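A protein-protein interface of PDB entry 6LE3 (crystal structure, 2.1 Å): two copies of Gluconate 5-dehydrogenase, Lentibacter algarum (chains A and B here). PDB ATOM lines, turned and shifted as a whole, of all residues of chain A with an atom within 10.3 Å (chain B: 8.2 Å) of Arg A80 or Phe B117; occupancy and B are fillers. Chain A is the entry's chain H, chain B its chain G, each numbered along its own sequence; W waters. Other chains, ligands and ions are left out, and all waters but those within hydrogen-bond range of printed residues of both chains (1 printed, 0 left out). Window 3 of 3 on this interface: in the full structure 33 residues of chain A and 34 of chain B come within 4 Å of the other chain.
Positions printed for both chains: 121 and 124.
The indole nitrogen (NE1) of Trp B120 lies within hydrogen-bond range of the side-chain hydroxyl (OG) of Ser A129 (2.9 Å).
OD1 of Asp B121 lies within salt-bridge range of NH2 of Arg A80, 2.8 Å away.
Of the 12 printed residues of chain B, 5 touch a printed residue of chain A.
Printed residues of chain B that touch a printed residue of chain A: Val B115, Phe B117, Trp B120, Asp B121 and Leu B124.
Hydrophobic or aromatic side chains of chain B within 4 Å of the printed part of chain A: Val B115, Phe B117, Trp B120 and Leu B124.
Of the 26 printed residues of chain A, 6 touch a printed residue of chain B.
Hydrophobic or aromatic side chains of chain A within 4 Å of the printed part of chain B: Phe A132 and Phe A133.
Arg A80 touches just these residues of chain B: Phe B117 (3.4 Å) and Asp B121 (2.4 Å).
Val A87 touches none of the printed residues of chain B.
Of the printed residues of chain B, Ser A129 touches Trp B120 (2.9 Å) and Leu B124 (3.5 Å).
Of chain A, only Arg A80 and Phe A133 come within 4 Å of Phe B117.
No residue of chain A comes within 4 Å of Asn B118.
No residue of chain A comes within 4 Å of Gly B119.
Printed residues of chain A within 4 Å of Leu B124: Ser A129 (3.5 Å).
The nearest residue of chain B that does not touch Arg A80 is Trp B120 (4.6 Å).
The nearest printed residue of chain B that does not touch Phe A133 is Val B115 (4.1 Å).
Phe B117 touches Arg A80 (CD1 to NE, 3.4 Å).
CZ2 of Trp B120 touches O of Leu A128 (3.9 Å).
Ser A129 touches Leu B124 (OG to CD2, 3.5 Å).
Val B115 touches Phe A132.
CB of Phe A132 touches CH2 of Trp B120 (3.7 Å).
Phe A133 touches Phe B117 (CD1 to CE1, 3.7 Å).
Trp B120 touches Phe A133 (CG to CZ, 3.6 Å).
O of Val B115 touches CE of Lys A136, at 3.5 Å.
The backbone NH of Ser A129 is in hydrogen-bond range of the backbone carbonyl oxygen of Leu A124.
Water W1 lies within hydrogen-bond range of NZ of Lys A136 (3.1 Å), O of Val B115 (3.3 Å) and O of Asp B114 (3.4 Å).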
ATOM      1  N   ALA A  75     -21.337  -6.571  36.616  1.00  0.00           N
ATOM      2  CA  ALA A  75     -21.612  -7.519  35.545  1.00  0.00           C
ATOM      3  C   ALA A  75     -21.696  -6.778  34.222  1.00  0.00           C
ATOM      4  O   ALA A  75     -21.989  -5.580  34.182  1.00  0.00           O
ATOM      5  CB  ALA A  75     -22.903  -8.312  35.795  1.00  0.00           C
ATOM      6  N   ASP A  76     -21.376  -7.495  33.150  1.00  0.00           N
ATOM      7  CA  ASP A  76     -21.621  -7.050  31.781  1.00  0.00           C
ATOM      8  C   ASP A  76     -22.938  -7.683  31.340  1.00  0.00           C
ATOM      9  O   ASP A  76     -22.971  -8.852  30.947  1.00  0.00           O
ATOM     10  CB  ASP A  76     -20.462  -7.457  30.880  1.00  0.00           C
ATOM     11  CG  ASP A  76     -20.718  -7.157  29.407  1.00  0.00           C
ATOM     12  OD1 ASP A  76     -21.747  -6.521  29.063  1.00  0.00           O
ATOM     13  OD2 ASP A  76     -19.879  -7.574  28.581  1.00  0.00           O
ATOM     14  N   VAL A  77     -24.030  -6.915  31.409  1.00  0.00           N
ATOM     15  CA  VAL A  77     -25.342  -7.488  31.120  1.00  0.00           C
ATOM     16  C   VAL A  77     -25.525  -7.852  29.656  1.00  0.00           C
ATOM     17  O   VAL A  77     -26.496  -8.543  29.323  1.00  0.00           O
ATOM     18  CB  VAL A  77     -26.491  -6.553  31.551  1.00  0.00           C
ATOM     19  CG1 VAL A  77     -26.433  -6.296  33.064  1.00  0.00           C
ATOM     20  CG2 VAL A  77     -26.469  -5.274  30.740  1.00  0.00           C
ATOM     21  N   ALA A  78     -24.645  -7.387  28.768  1.00  0.00           N
ATOM     22  CA  ALA A  78     -24.703  -7.818  27.375  1.00  0.00           C
ATOM     23  C   ALA A  78     -24.046  -9.175  27.152  1.00  0.00           C
ATOM     24  O   ALA A  78     -24.233  -9.768  26.083  1.00  0.00           O
ATOM     25  CB  ALA A  78     -24.047  -6.778  26.460  1.00  0.00           C
ATOM     26  N   SER A  79     -23.287  -9.671  28.128  1.00  0.00           N
ATOM     27  CA  SER A  79     -22.544 -10.913  27.975  1.00  0.00           C
ATOM     28  C   SER A  79     -23.477 -12.115  28.056  1.00  0.00           C
ATOM     29  O   SER A  79     -24.147 -12.322  29.069  1.00  0.00           O
ATOM     30  CB  SER A  79     -21.460 -11.013  29.043  1.00  0.00           C
ATOM     31  OG  SER A  79     -20.758 -12.222  28.885  1.00  0.00           O
ATOM     32  N   ARG A  80     -23.481 -12.935  27.011  1.00  0.00           N
ATOM     33  CA  ARG A  80     -24.331 -14.119  27.007  1.00  0.00           C
ATOM     34  C   ARG A  80     -23.854 -15.147  28.031  1.00  0.00           C
ATOM     35  O   ARG A  80     -24.647 -15.644  28.837  1.00  0.00           O
ATOM     36  CB  ARG A  80     -24.353 -14.714  25.598  1.00  0.00           C
ATOM     37  CG  ARG A  80     -25.423 -15.734  25.395  1.00  0.00           C
ATOM     38  CD  ARG A  80     -25.798 -15.820  23.931  1.00  0.00           C
ATOM     39  NE  ARG A  80     -26.592 -14.678  23.475  1.00  0.00           N
ATOM     40  CZ  ARG A  80     -26.966 -14.516  22.209  1.00  0.00           C
ATOM     41  NH1 ARG A  80     -26.611 -15.420  21.304  1.00  0.00           N
ATOM     42  NH2 ARG A  80     -27.690 -13.461  21.853  1.00  0.00           N
ATOM     43  N   ASP A  81     -22.550 -15.436  28.048  1.00  0.00           N
ATOM     44  CA  ASP A  81     -21.981 -16.332  29.056  1.00  0.00           C
ATOM     45  C   ASP A  81     -22.320 -15.891  30.475  1.00  0.00           C
ATOM     46  O   ASP A  81     -22.545 -16.728  31.358  1.00  0.00           O
ATOM     47  CB  ASP A  81     -20.461 -16.402  28.894  1.00  0.00           C
ATOM     48  CG  ASP A  81     -20.041 -17.219  27.686  1.00  0.00           C
ATOM     49  OD1 ASP A  81     -20.938 -17.783  27.030  1.00  0.00           O
ATOM     50  OD2 ASP A  81     -18.821 -17.288  27.388  1.00  0.00           O
ATOM     51  N   GLY A  82     -22.324 -14.583  30.727  1.00  0.00           N
ATOM     52  CA  GLY A  82     -22.530 -14.084  32.077  1.00  0.00           C
ATOM     53  C   GLY A  82     -23.954 -14.116  32.596  1.00  0.00           C
ATOM     54  O   GLY A  82     -24.151 -13.887  33.792  1.00  0.00           O
ATOM     55  N   LEU A  83     -24.947 -14.410  31.748  1.00  0.00           N
ATOM     56  CA  LEU A  83     -26.339 -14.147  32.118  1.00  0.00           C
ATOM     57  C   LEU A  83     -26.747 -14.904  33.376  1.00  0.00           C
ATOM     58  O   LEU A  83     -27.294 -14.312  34.309  1.00  0.00           O
ATOM     59  CB  LEU A  83     -27.277 -14.494  30.961  1.00  0.00           C
ATOM     60  CG  LEU A  83     -28.763 -14.124  31.068  1.00  0.00           C
ATOM     61  CD1 LEU A  83     -28.980 -12.608  31.194  1.00  0.00           C
ATOM     62  CD2 LEU A  83     -29.501 -14.643  29.846  1.00  0.00           C
ATOM     63  N   GLU A  84     -26.504 -16.219  33.412  1.00  0.00           N
ATOM     64  CA  GLU A  84     -26.917 -17.028  34.558  1.00  0.00           C
ATOM     65  C   GLU A  84     -26.327 -16.500  35.861  1.00  0.00           C
ATOM     66  O   GLU A  84     -27.051 -16.289  36.846  1.00  0.00           O
ATOM     67  CB  GLU A  84     -26.501 -18.482  34.348  1.00  0.00           C
ATOM     68  CG  GLU A  84     -26.193 -19.211  35.660  1.00  0.00           C
ATOM     69  CD  GLU A  84     -26.064 -20.706  35.489  1.00  0.00           C
ATOM     70  OE1 GLU A  84     -25.070 -21.153  34.877  1.00  0.00           O
ATOM     71  OE2 GLU A  84     -26.956 -21.433  35.972  1.00  0.00           O
ATOM     72  N   ARG A  85     -25.019 -16.246  35.874  1.00  0.00           N
ATOM     73  CA  ARG A  85     -24.382 -15.740  37.088  1.00  0.00           C
ATOM     74  C   ARG A  85     -24.851 -14.326  37.424  1.00  0.00           C
ATOM     75  O   ARG A  85     -25.033 -13.999  38.605  1.00  0.00           O
ATOM     76  CB  ARG A  85     -22.860 -15.785  36.961  1.00  0.00           C
ATOM     77  CG  ARG A  85     -22.138 -15.403  38.250  1.00  0.00           C
ATOM     78  CD  ARG A  85     -20.645 -15.293  37.999  1.00  0.00           C
ATOM     79  NE  ARG A  85     -19.984 -14.303  38.853  1.00  0.00           N
ATOM     80  CZ  ARG A  85     -19.072 -14.597  39.775  1.00  0.00           C
ATOM     81  NH1 ARG A  85     -18.707 -15.862  39.968  1.00  0.00           N
ATOM     82  NH2 ARG A  85     -18.523 -13.629  40.495  1.00  0.00           N
ATOM     83  N   THR A  86     -24.986 -13.458  36.409  1.00  0.00           N
ATOM     84  CA  THR A  86     -25.524 -12.112  36.626  1.00  0.00           C
ATOM     85  C   THR A  86     -26.873 -12.180  37.327  1.00  0.00           C
ATOM     86  O   THR A  86     -27.126 -11.441  38.285  1.00  0.00           O
ATOM     87  CB  THR A  86     -25.657 -11.375  35.282  1.00  0.00           C
ATOM     88  OG1 THR A  86     -24.370 -11.193  34.687  1.00  0.00           O
ATOM     89  CG2 THR A  86     -26.318 -10.005  35.441  1.00  0.00           C
ATOM     90  N   VAL A  87     -27.735 -13.097  36.882  1.00  0.00           N
ATOM     91  CA  VAL A  87     -29.065 -13.245  37.462  1.00  0.00           C
ATOM     92  C   VAL A  87     -28.963 -13.710  38.909  1.00  0.00           C
ATOM     93  O   VAL A  87     -29.651 -13.181  39.798  1.00  0.00           O
ATOM     94  CB  VAL A  87     -29.911 -14.207  36.601  1.00  0.00           C
ATOM     95  CG1 VAL A  87     -31.172 -14.605  37.333  1.00  0.00           C
ATOM     96  CG2 VAL A  87     -30.277 -13.555  35.256  1.00  0.00           C
ATOM     97  N   ASP A 121     -22.758  -4.232  16.411  1.00  0.00           N
ATOM     98  CA  ASP A 121     -23.064  -5.405  17.233  1.00  0.00           C
ATOM     99  C   ASP A 121     -23.119  -5.057  18.711  1.00  0.00           C
ATOM    100  O   ASP A 121     -23.973  -5.572  19.434  1.00  0.00           O
ATOM    101  CB  ASP A 121     -22.040  -6.525  17.023  1.00  0.00           C
ATOM    102  CG  ASP A 121     -22.067  -7.110  15.614  1.00  0.00           C
ATOM    103  OD1 ASP A 121     -23.042  -6.887  14.861  1.00  0.00           O
ATOM    104  OD2 ASP A 121     -21.085  -7.803  15.261  1.00  0.00           O
ATOM    105  N   LEU A 124     -26.530  -3.258  19.362  1.00  0.00           N
ATOM    106  CA  LEU A 124     -27.668  -4.175  19.401  1.00  0.00           C
ATOM    107  C   LEU A 124     -27.611  -5.074  20.627  1.00  0.00           C
ATOM    108  O   LEU A 124     -28.634  -5.297  21.281  1.00  0.00           O
ATOM    109  CB  LEU A 124     -27.753  -5.005  18.121  1.00  0.00           C
ATOM    110  CG  LEU A 124     -28.597  -4.395  16.986  1.00  0.00           C
ATOM    111  CD1 LEU A 124     -27.975  -3.097  16.460  1.00  0.00           C
ATOM    112  CD2 LEU A 124     -28.816  -5.389  15.841  1.00  0.00           C
ATOM    113  N   ALA A 125     -26.421  -5.580  20.981  1.00  0.00           N
ATOM    114  CA  ALA A 125     -26.320  -6.475  22.133  1.00  0.00           C
ATOM    115  C   ALA A 125     -26.723  -5.784  23.434  1.00  0.00           C
ATOM    116  O   ALA A 125     -27.409  -6.384  24.270  1.00  0.00           O
ATOM    117  CB  ALA A 125     -24.901  -7.037  22.243  1.00  0.00           C
ATOM    118  N   LEU A 126     -26.283  -4.539  23.648  1.00  0.00           N
ATOM    119  CA  LEU A 126     -26.598  -3.898  24.928  1.00  0.00           C
ATOM    120  C   LEU A 126     -28.001  -3.285  24.958  1.00  0.00           C
ATOM    121  O   LEU A 126     -28.690  -3.377  25.977  1.00  0.00           O
ATOM    122  CB  LEU A 126     -25.554  -2.829  25.276  1.00  0.00           C
ATOM    123  CG  LEU A 126     -25.744  -2.121  26.640  1.00  0.00           C
ATOM    124  CD1 LEU A 126     -25.886  -3.127  27.785  1.00  0.00           C
ATOM    125  CD2 LEU A 126     -24.607  -1.127  26.946  1.00  0.00           C
ATOM    126  N   LEU A 128     -30.819  -3.769  22.930  1.00  0.00           N
ATOM    127  CA  LEU A 128     -31.984  -4.543  22.504  1.00  0.00           C
ATOM    128  C   LEU A 128     -31.981  -5.949  23.081  1.00  0.00           C
ATOM    129  O   LEU A 128     -32.942  -6.335  23.768  1.00  0.00           O
ATOM    130  CB  LEU A 128     -32.042  -4.590  20.961  1.00  0.00           C
ATOM    131  CG  LEU A 128     -33.386  -4.799  20.231  1.00  0.00           C
ATOM    132  CD1 LEU A 128     -34.470  -3.874  20.781  1.00  0.00           C
ATOM    133  CD2 LEU A 128     -33.253  -4.628  18.677  1.00  0.00           C
ATOM    134  N   SER A 129     -30.898  -6.709  22.879  1.00  0.00           N
ATOM    135  CA  SER A 129     -30.889  -8.116  23.278  1.00  0.00           C
ATOM    136  C   SER A 129     -30.802  -8.259  24.799  1.00  0.00           C
ATOM    137  O   SER A 129     -31.520  -9.075  25.408  1.00  0.00           O
ATOM    138  CB  SER A 129     -29.728  -8.845  22.584  1.00  0.00           C
ATOM    139  OG  SER A 129     -29.739  -8.603  21.178  1.00  0.00           O
ATOM    140  N   ALA A 130     -29.913  -7.487  25.425  1.00  0.00           N
ATOM    141  CA  ALA A 130     -29.760  -7.558  26.878  1.00  0.00           C
ATOM    142  C   ALA A 130     -31.064  -7.309  27.622  1.00  0.00           C
ATOM    143  O   ALA A 130     -31.402  -8.123  28.498  1.00  0.00           O
ATOM    144  CB  ALA A 130     -28.657  -6.597  27.343  1.00  0.00           C
ATOM    145  N   PRO A 131     -31.827  -6.229  27.369  1.00  0.00           N
ATOM    146  CA  PRO A 131     -33.081  -6.063  28.130  1.00  0.00           C
ATOM    147  C   PRO A 131     -34.025  -7.243  27.984  1.00  0.00           C
ATOM    148  O   PRO A 131     -34.672  -7.640  28.966  1.00  0.00           O
ATOM    149  CB  PRO A 131     -33.694  -4.781  27.548  1.00  0.00           C
ATOM    150  CG  PRO A 131     -32.580  -4.099  26.865  1.00  0.00           C
ATOM    151  CD  PRO A 131     -31.592  -5.102  26.445  1.00  0.00           C
ATOM    152  N   PHE A 132     -34.091  -7.838  26.788  1.00  0.00           N
ATOM    153  CA  PHE A 132     -34.999  -8.960  26.595  1.00  0.00           C
ATOM    154  C   PHE A 132     -34.571 -10.166  27.415  1.00  0.00           C
ATOM    155  O   PHE A 132     -35.382 -10.742  28.141  1.00  0.00           O
ATOM    156  CB  PHE A 132     -35.117  -9.372  25.131  1.00  0.00           C
ATOM    157  CG  PHE A 132     -35.887 -10.669  24.971  1.00  0.00           C
ATOM    158  CD1 PHE A 132     -37.252 -10.712  25.254  1.00  0.00           C
ATOM    159  CD2 PHE A 132     -35.238 -11.857  24.649  1.00  0.00           C
ATOM    160  CE1 PHE A 132     -37.968 -11.908  25.158  1.00  0.00           C
ATOM    161  CE2 PHE A 132     -35.946 -13.055  24.544  1.00  0.00           C
ATOM    162  CZ  PHE A 132     -37.319 -13.079  24.790  1.00  0.00           C
ATOM    163  N   PHE A 133     -33.315 -10.602  27.267  1.00  0.00           N
ATOM    164  CA  PHE A 133     -32.909 -11.814  27.979  1.00  0.00           C
ATOM    165  C   PHE A 133     -32.842 -11.600  29.498  1.00  0.00           C
ATOM    166  O   PHE A 133     -33.213 -12.498  30.262  1.00  0.00           O
ATOM    167  CB  PHE A 133     -31.612 -12.359  27.369  1.00  0.00           C
ATOM    168  CG  PHE A 133     -31.815 -12.927  25.974  1.00  0.00           C
ATOM    169  CD1 PHE A 133     -32.445 -14.158  25.794  1.00  0.00           C
ATOM    170  CD2 PHE A 133     -31.468 -12.184  24.847  1.00  0.00           C
ATOM    171  CE1 PHE A 133     -32.674 -14.649  24.526  1.00  0.00           C
ATOM    172  CE2 PHE A 133     -31.687 -12.664  23.580  1.00  0.00           C
ATOM    173  CZ  PHE A 133     -32.293 -13.905  23.411  1.00  0.00           C
ATOM    174  N   LEU A 134     -32.471 -10.408  29.968  1.00  0.00           N
ATOM    175  CA  LEU A 134     -32.517 -10.165  31.411  1.00  0.00           C
ATOM    176  C   LEU A 134     -33.957 -10.202  31.942  1.00  0.00           C
ATOM    177  O   LEU A 134     -34.245 -10.855  32.967  1.00  0.00           O
ATOM    178  CB  LEU A 134     -31.850  -8.824  31.727  1.00  0.00           C
ATOM    179  CG  LEU A 134     -31.136  -8.687  33.075  1.00  0.00           C
ATOM    180  CD1 LEU A 134     -30.220  -9.888  33.362  1.00  0.00           C
ATOM    181  CD2 LEU A 134     -30.366  -7.364  33.131  1.00  0.00           C
ATOM    182  N   LYS A 136     -36.492 -11.747  30.609  1.00  0.00           N
ATOM    183  CA  LYS A 136     -36.960 -13.116  30.461  1.00  0.00           C
ATOM    184  C   LYS A 136     -36.477 -13.977  31.617  1.00  0.00           C
ATOM    185  O   LYS A 136     -37.232 -14.799  32.142  1.00  0.00           O
ATOM    186  CB  LYS A 136     -36.487 -13.665  29.110  1.00  0.00           C
ATOM    187  CG  LYS A 136     -36.781 -15.141  28.817  1.00  0.00           C
ATOM    188  CD  LYS A 136     -36.162 -15.505  27.449  1.00  0.00           C
ATOM    189  CE  LYS A 136     -35.680 -16.961  27.362  1.00  0.00           C
ATOM    190  NZ  LYS A 136     -36.466 -17.906  28.186  1.00  0.00           N
ATOM    191  N   ALA A 137     -35.226 -13.780  32.044  1.00  0.00           N
ATOM    192  CA  ALA A 137     -34.727 -14.490  33.219  1.00  0.00           C
ATOM    193  C   ALA A 137     -35.515 -14.123  34.470  1.00  0.00           C
ATOM    194  O   ALA A 137     -35.711 -14.966  35.346  1.00  0.00           O
ATOM    195  CB  ALA A 137     -33.239 -14.199  33.427  1.00  0.00           C
ATOM    196  N   GLU B 110     -41.211 -17.826  17.938  1.00  0.00           N
ATOM    197  CA  GLU B 110     -40.964 -18.200  19.332  1.00  0.00           C
ATOM    198  C   GLU B 110     -41.601 -17.167  20.268  1.00  0.00           C
ATOM    199  O   GLU B 110     -41.258 -15.980  20.215  1.00  0.00           O
ATOM    200  CB  GLU B 110     -39.457 -18.296  19.589  1.00  0.00           C
ATOM    201  CG  GLU B 110     -38.716 -19.456  18.910  1.00  0.00           C
ATOM    202  CD  GLU B 110     -37.174 -19.388  19.095  1.00  0.00           C
ATOM    203  OE1 GLU B 110     -36.631 -18.323  19.486  1.00  0.00           O
ATOM    204  OE2 GLU B 110     -36.504 -20.411  18.837  1.00  0.00           O
ATOM    205  N   ASP B 114     -40.240 -18.796  25.289  1.00  0.00           N
ATOM    206  CA  ASP B 114     -39.591 -19.868  24.544  1.00  0.00           C
ATOM    207  C   ASP B 114     -38.431 -19.390  23.679  1.00  0.00           C
ATOM    208  O   ASP B 114     -37.816 -20.213  22.996  1.00  0.00           O
ATOM    209  CB  ASP B 114     -40.609 -20.591  23.658  1.00  0.00           C
ATOM    210  CG  ASP B 114     -41.843 -21.018  24.426  1.00  0.00           C
ATOM    211  OD1 ASP B 114     -41.683 -21.634  25.499  1.00  0.00           O
ATOM    212  OD2 ASP B 114     -42.966 -20.694  23.977  1.00  0.00           O
ATOM    213  N   VAL B 115     -38.098 -18.097  23.700  1.00  0.00           N
ATOM    214  CA  VAL B 115     -37.095 -17.580  22.769  1.00  0.00           C
ATOM    215  C   VAL B 115     -35.731 -18.195  23.044  1.00  0.00           C
ATOM    216  O   VAL B 115     -35.294 -18.301  24.195  1.00  0.00           O
ATOM    217  CB  VAL B 115     -37.038 -16.047  22.826  1.00  0.00           C
ATOM    218  CG1 VAL B 115     -35.799 -15.537  22.063  1.00  0.00           C
ATOM    219  CG2 VAL B 115     -38.303 -15.475  22.220  1.00  0.00           C
ATOM    220  N   THR B 116     -35.055 -18.616  21.975  1.00  0.00           N
ATOM    221  CA  THR B 116     -33.690 -19.122  22.030  1.00  0.00           C
ATOM    222  C   THR B 116     -32.722 -18.059  21.528  1.00  0.00           C
ATOM    223  O   THR B 116     -33.092 -17.139  20.786  1.00  0.00           O
ATOM    224  CB  THR B 116     -33.511 -20.400  21.192  1.00  0.00           C
ATOM    225  OG1 THR B 116     -33.772 -20.118  19.810  1.00  0.00           O
ATOM    226  CG2 THR B 116     -34.461 -21.507  21.665  1.00  0.00           C
ATOM    227  N   PHE B 117     -31.466 -18.195  21.967  1.00  0.00           N
ATOM    228  CA  PHE B 117     -30.395 -17.358  21.444  1.00  0.00           C
ATOM    229  C   PHE B 117     -30.339 -17.417  19.928  1.00  0.00           C
ATOM    230  O   PHE B 117     -30.207 -16.385  19.262  1.00  0.00           O
ATOM    231  CB  PHE B 117     -29.061 -17.800  22.042  1.00  0.00           C
ATOM    232  CG  PHE B 117     -28.943 -17.520  23.498  1.00  0.00           C
ATOM    233  CD1 PHE B 117     -29.448 -16.346  24.029  1.00  0.00           C
ATOM    234  CD2 PHE B 117     -28.330 -18.427  24.340  1.00  0.00           C
ATOM    235  CE1 PHE B 117     -29.337 -16.078  25.375  1.00  0.00           C
ATOM    236  CE2 PHE B 117     -28.216 -18.169  25.690  1.00  0.00           C
ATOM    237  CZ  PHE B 117     -28.724 -16.993  26.209  1.00  0.00           C
ATOM    238  N   ASN B 118     -30.449 -18.623  19.364  1.00  0.00           N
ATOM    239  CA  ASN B 118     -30.278 -18.783  17.925  1.00  0.00           C
ATOM    240  C   ASN B 118     -31.447 -18.172  17.158  1.00  0.00           C
ATOM    241  O   ASN B 118     -31.238 -17.487  16.158  1.00  0.00           O
ATOM    242  CB  ASN B 118     -30.110 -20.262  17.569  1.00  0.00           C
ATOM    243  CG  ASN B 118     -28.749 -20.822  17.997  1.00  0.00           C
ATOM    244  OD1 ASN B 118     -27.865 -20.077  18.428  1.00  0.00           O
ATOM    245  ND2 ASN B 118     -28.586 -22.143  17.894  1.00  0.00           N
ATOM    246  N   GLY B 119     -32.681 -18.386  17.627  1.00  0.00           N
ATOM    247  CA  GLY B 119     -33.830 -17.768  16.977  1.00  0.00           C
ATOM    248  C   GLY B 119     -33.771 -16.249  17.022  1.00  0.00           C
ATOM    249  O   GLY B 119     -33.995 -15.570  16.013  1.00  0.00           O
ATOM    250  N   TRP B 120     -33.458 -15.700  18.199  1.00  0.00           N
ATOM    251  CA  TRP B 120     -33.320 -14.252  18.353  1.00  0.00           C
ATOM    252  C   TRP B 120     -32.225 -13.697  17.452  1.00  0.00           C
ATOM    253  O   TRP B 120     -32.465 -12.764  16.678  1.00  0.00           O
ATOM    254  CB  TRP B 120     -33.042 -13.921  19.817  1.00  0.00           C
ATOM    255  CG  TRP B 120     -32.789 -12.463  20.122  1.00  0.00           C
ATOM    256  CD1 TRP B 120     -31.579 -11.799  20.059  1.00  0.00           C
ATOM    257  CD2 TRP B 120     -33.752 -11.498  20.578  1.00  0.00           C
ATOM    258  NE1 TRP B 120     -31.751 -10.486  20.431  1.00  0.00           N
ATOM    259  CE2 TRP B 120     -33.069 -10.274  20.751  1.00  0.00           C
ATOM    260  CE3 TRP B 120     -35.129 -11.546  20.844  1.00  0.00           C
ATOM    261  CZ2 TRP B 120     -33.713  -9.111  21.196  1.00  0.00           C
ATOM    262  CZ3 TRP B 120     -35.774 -10.382  21.270  1.00  0.00           C
ATOM    263  CH2 TRP B 120     -35.062  -9.187  21.451  1.00  0.00           C
ATOM    264  N   ASP B 121     -31.015 -14.274  17.533  1.00  0.00           N
ATOM    265  CA  ASP B 121     -29.886 -13.793  16.749  1.00  0.00           C
ATOM    266  C   ASP B 121     -30.161 -13.902  15.258  1.00  0.00           C
ATOM    267  O   ASP B 121     -29.805 -13.004  14.502  1.00  0.00           O
ATOM    268  CB  ASP B 121     -28.609 -14.559  17.104  1.00  0.00           C
ATOM    269  CG  ASP B 121     -28.188 -14.360  18.555  1.00  0.00           C
ATOM    270  OD1 ASP B 121     -28.711 -13.436  19.216  1.00  0.00           O
ATOM    271  OD2 ASP B 121     -27.336 -15.136  19.036  1.00  0.00           O
ATOM    272  N   GLN B 122     -30.808 -14.981  14.808  1.00  0.00           N
ATOM    273  CA  GLN B 122     -31.085 -15.094  13.380  1.00  0.00           C
ATOM    274  C   GLN B 122     -32.124 -14.055  12.932  1.00  0.00           C
ATOM    275  O   GLN B 122     -32.008 -13.475  11.844  1.00  0.00           O
ATOM    276  CB  GLN B 122     -31.525 -16.534  13.048  1.00  0.00           C
ATOM    277  CG  GLN B 122     -33.028 -16.764  13.147  1.00  0.00           C
ATOM    278  CD  GLN B 122     -33.512 -18.056  12.479  1.00  0.00           C
ATOM    279  OE1 GLN B 122     -33.526 -18.174  11.251  1.00  0.00           O
ATOM    280  NE2 GLN B 122     -33.936 -19.017  13.293  1.00  0.00           N
ATOM    281  N   THR B 123     -33.109 -13.758  13.781  1.00  0.00           N
ATOM    282  CA  THR B 123     -34.067 -12.707  13.448  1.00  0.00           C
ATOM    283  C   THR B 123     -33.386 -11.345  13.341  1.00  0.00           C
ATOM    284  O   THR B 123     -33.609 -10.601  12.378  1.00  0.00           O
ATOM    285  CB  THR B 123     -35.174 -12.659  14.489  1.00  0.00           C
ATOM    286  OG1 THR B 123     -35.734 -13.965  14.626  1.00  0.00           O
ATOM    287  CG2 THR B 123     -36.265 -11.654  14.070  1.00  0.00           C
ATOM    288  N   LEU B 124     -32.547 -11.004  14.324  1.00  0.00           N
ATOM    289  CA  LEU B 124     -31.849  -9.719  14.275  1.00  0.00           C
ATOM    290  C   LEU B 124     -30.902  -9.651  13.085  1.00  0.00           C
ATOM    291  O   LEU B 124     -30.878  -8.651  12.362  1.00  0.00           O
ATOM    292  CB  LEU B 124     -31.089  -9.467  15.581  1.00  0.00           C
ATOM    293  CG  LEU B 124     -31.812  -8.704  16.706  1.00  0.00           C
ATOM    294  CD1 LEU B 124     -33.100  -9.398  17.192  1.00  0.00           C
ATOM    295  CD2 LEU B 124     -30.850  -8.512  17.854  1.00  0.00           C
HETATM  296  O   HOH W   1     -36.807 -20.363  26.279  1.00  0.00           O
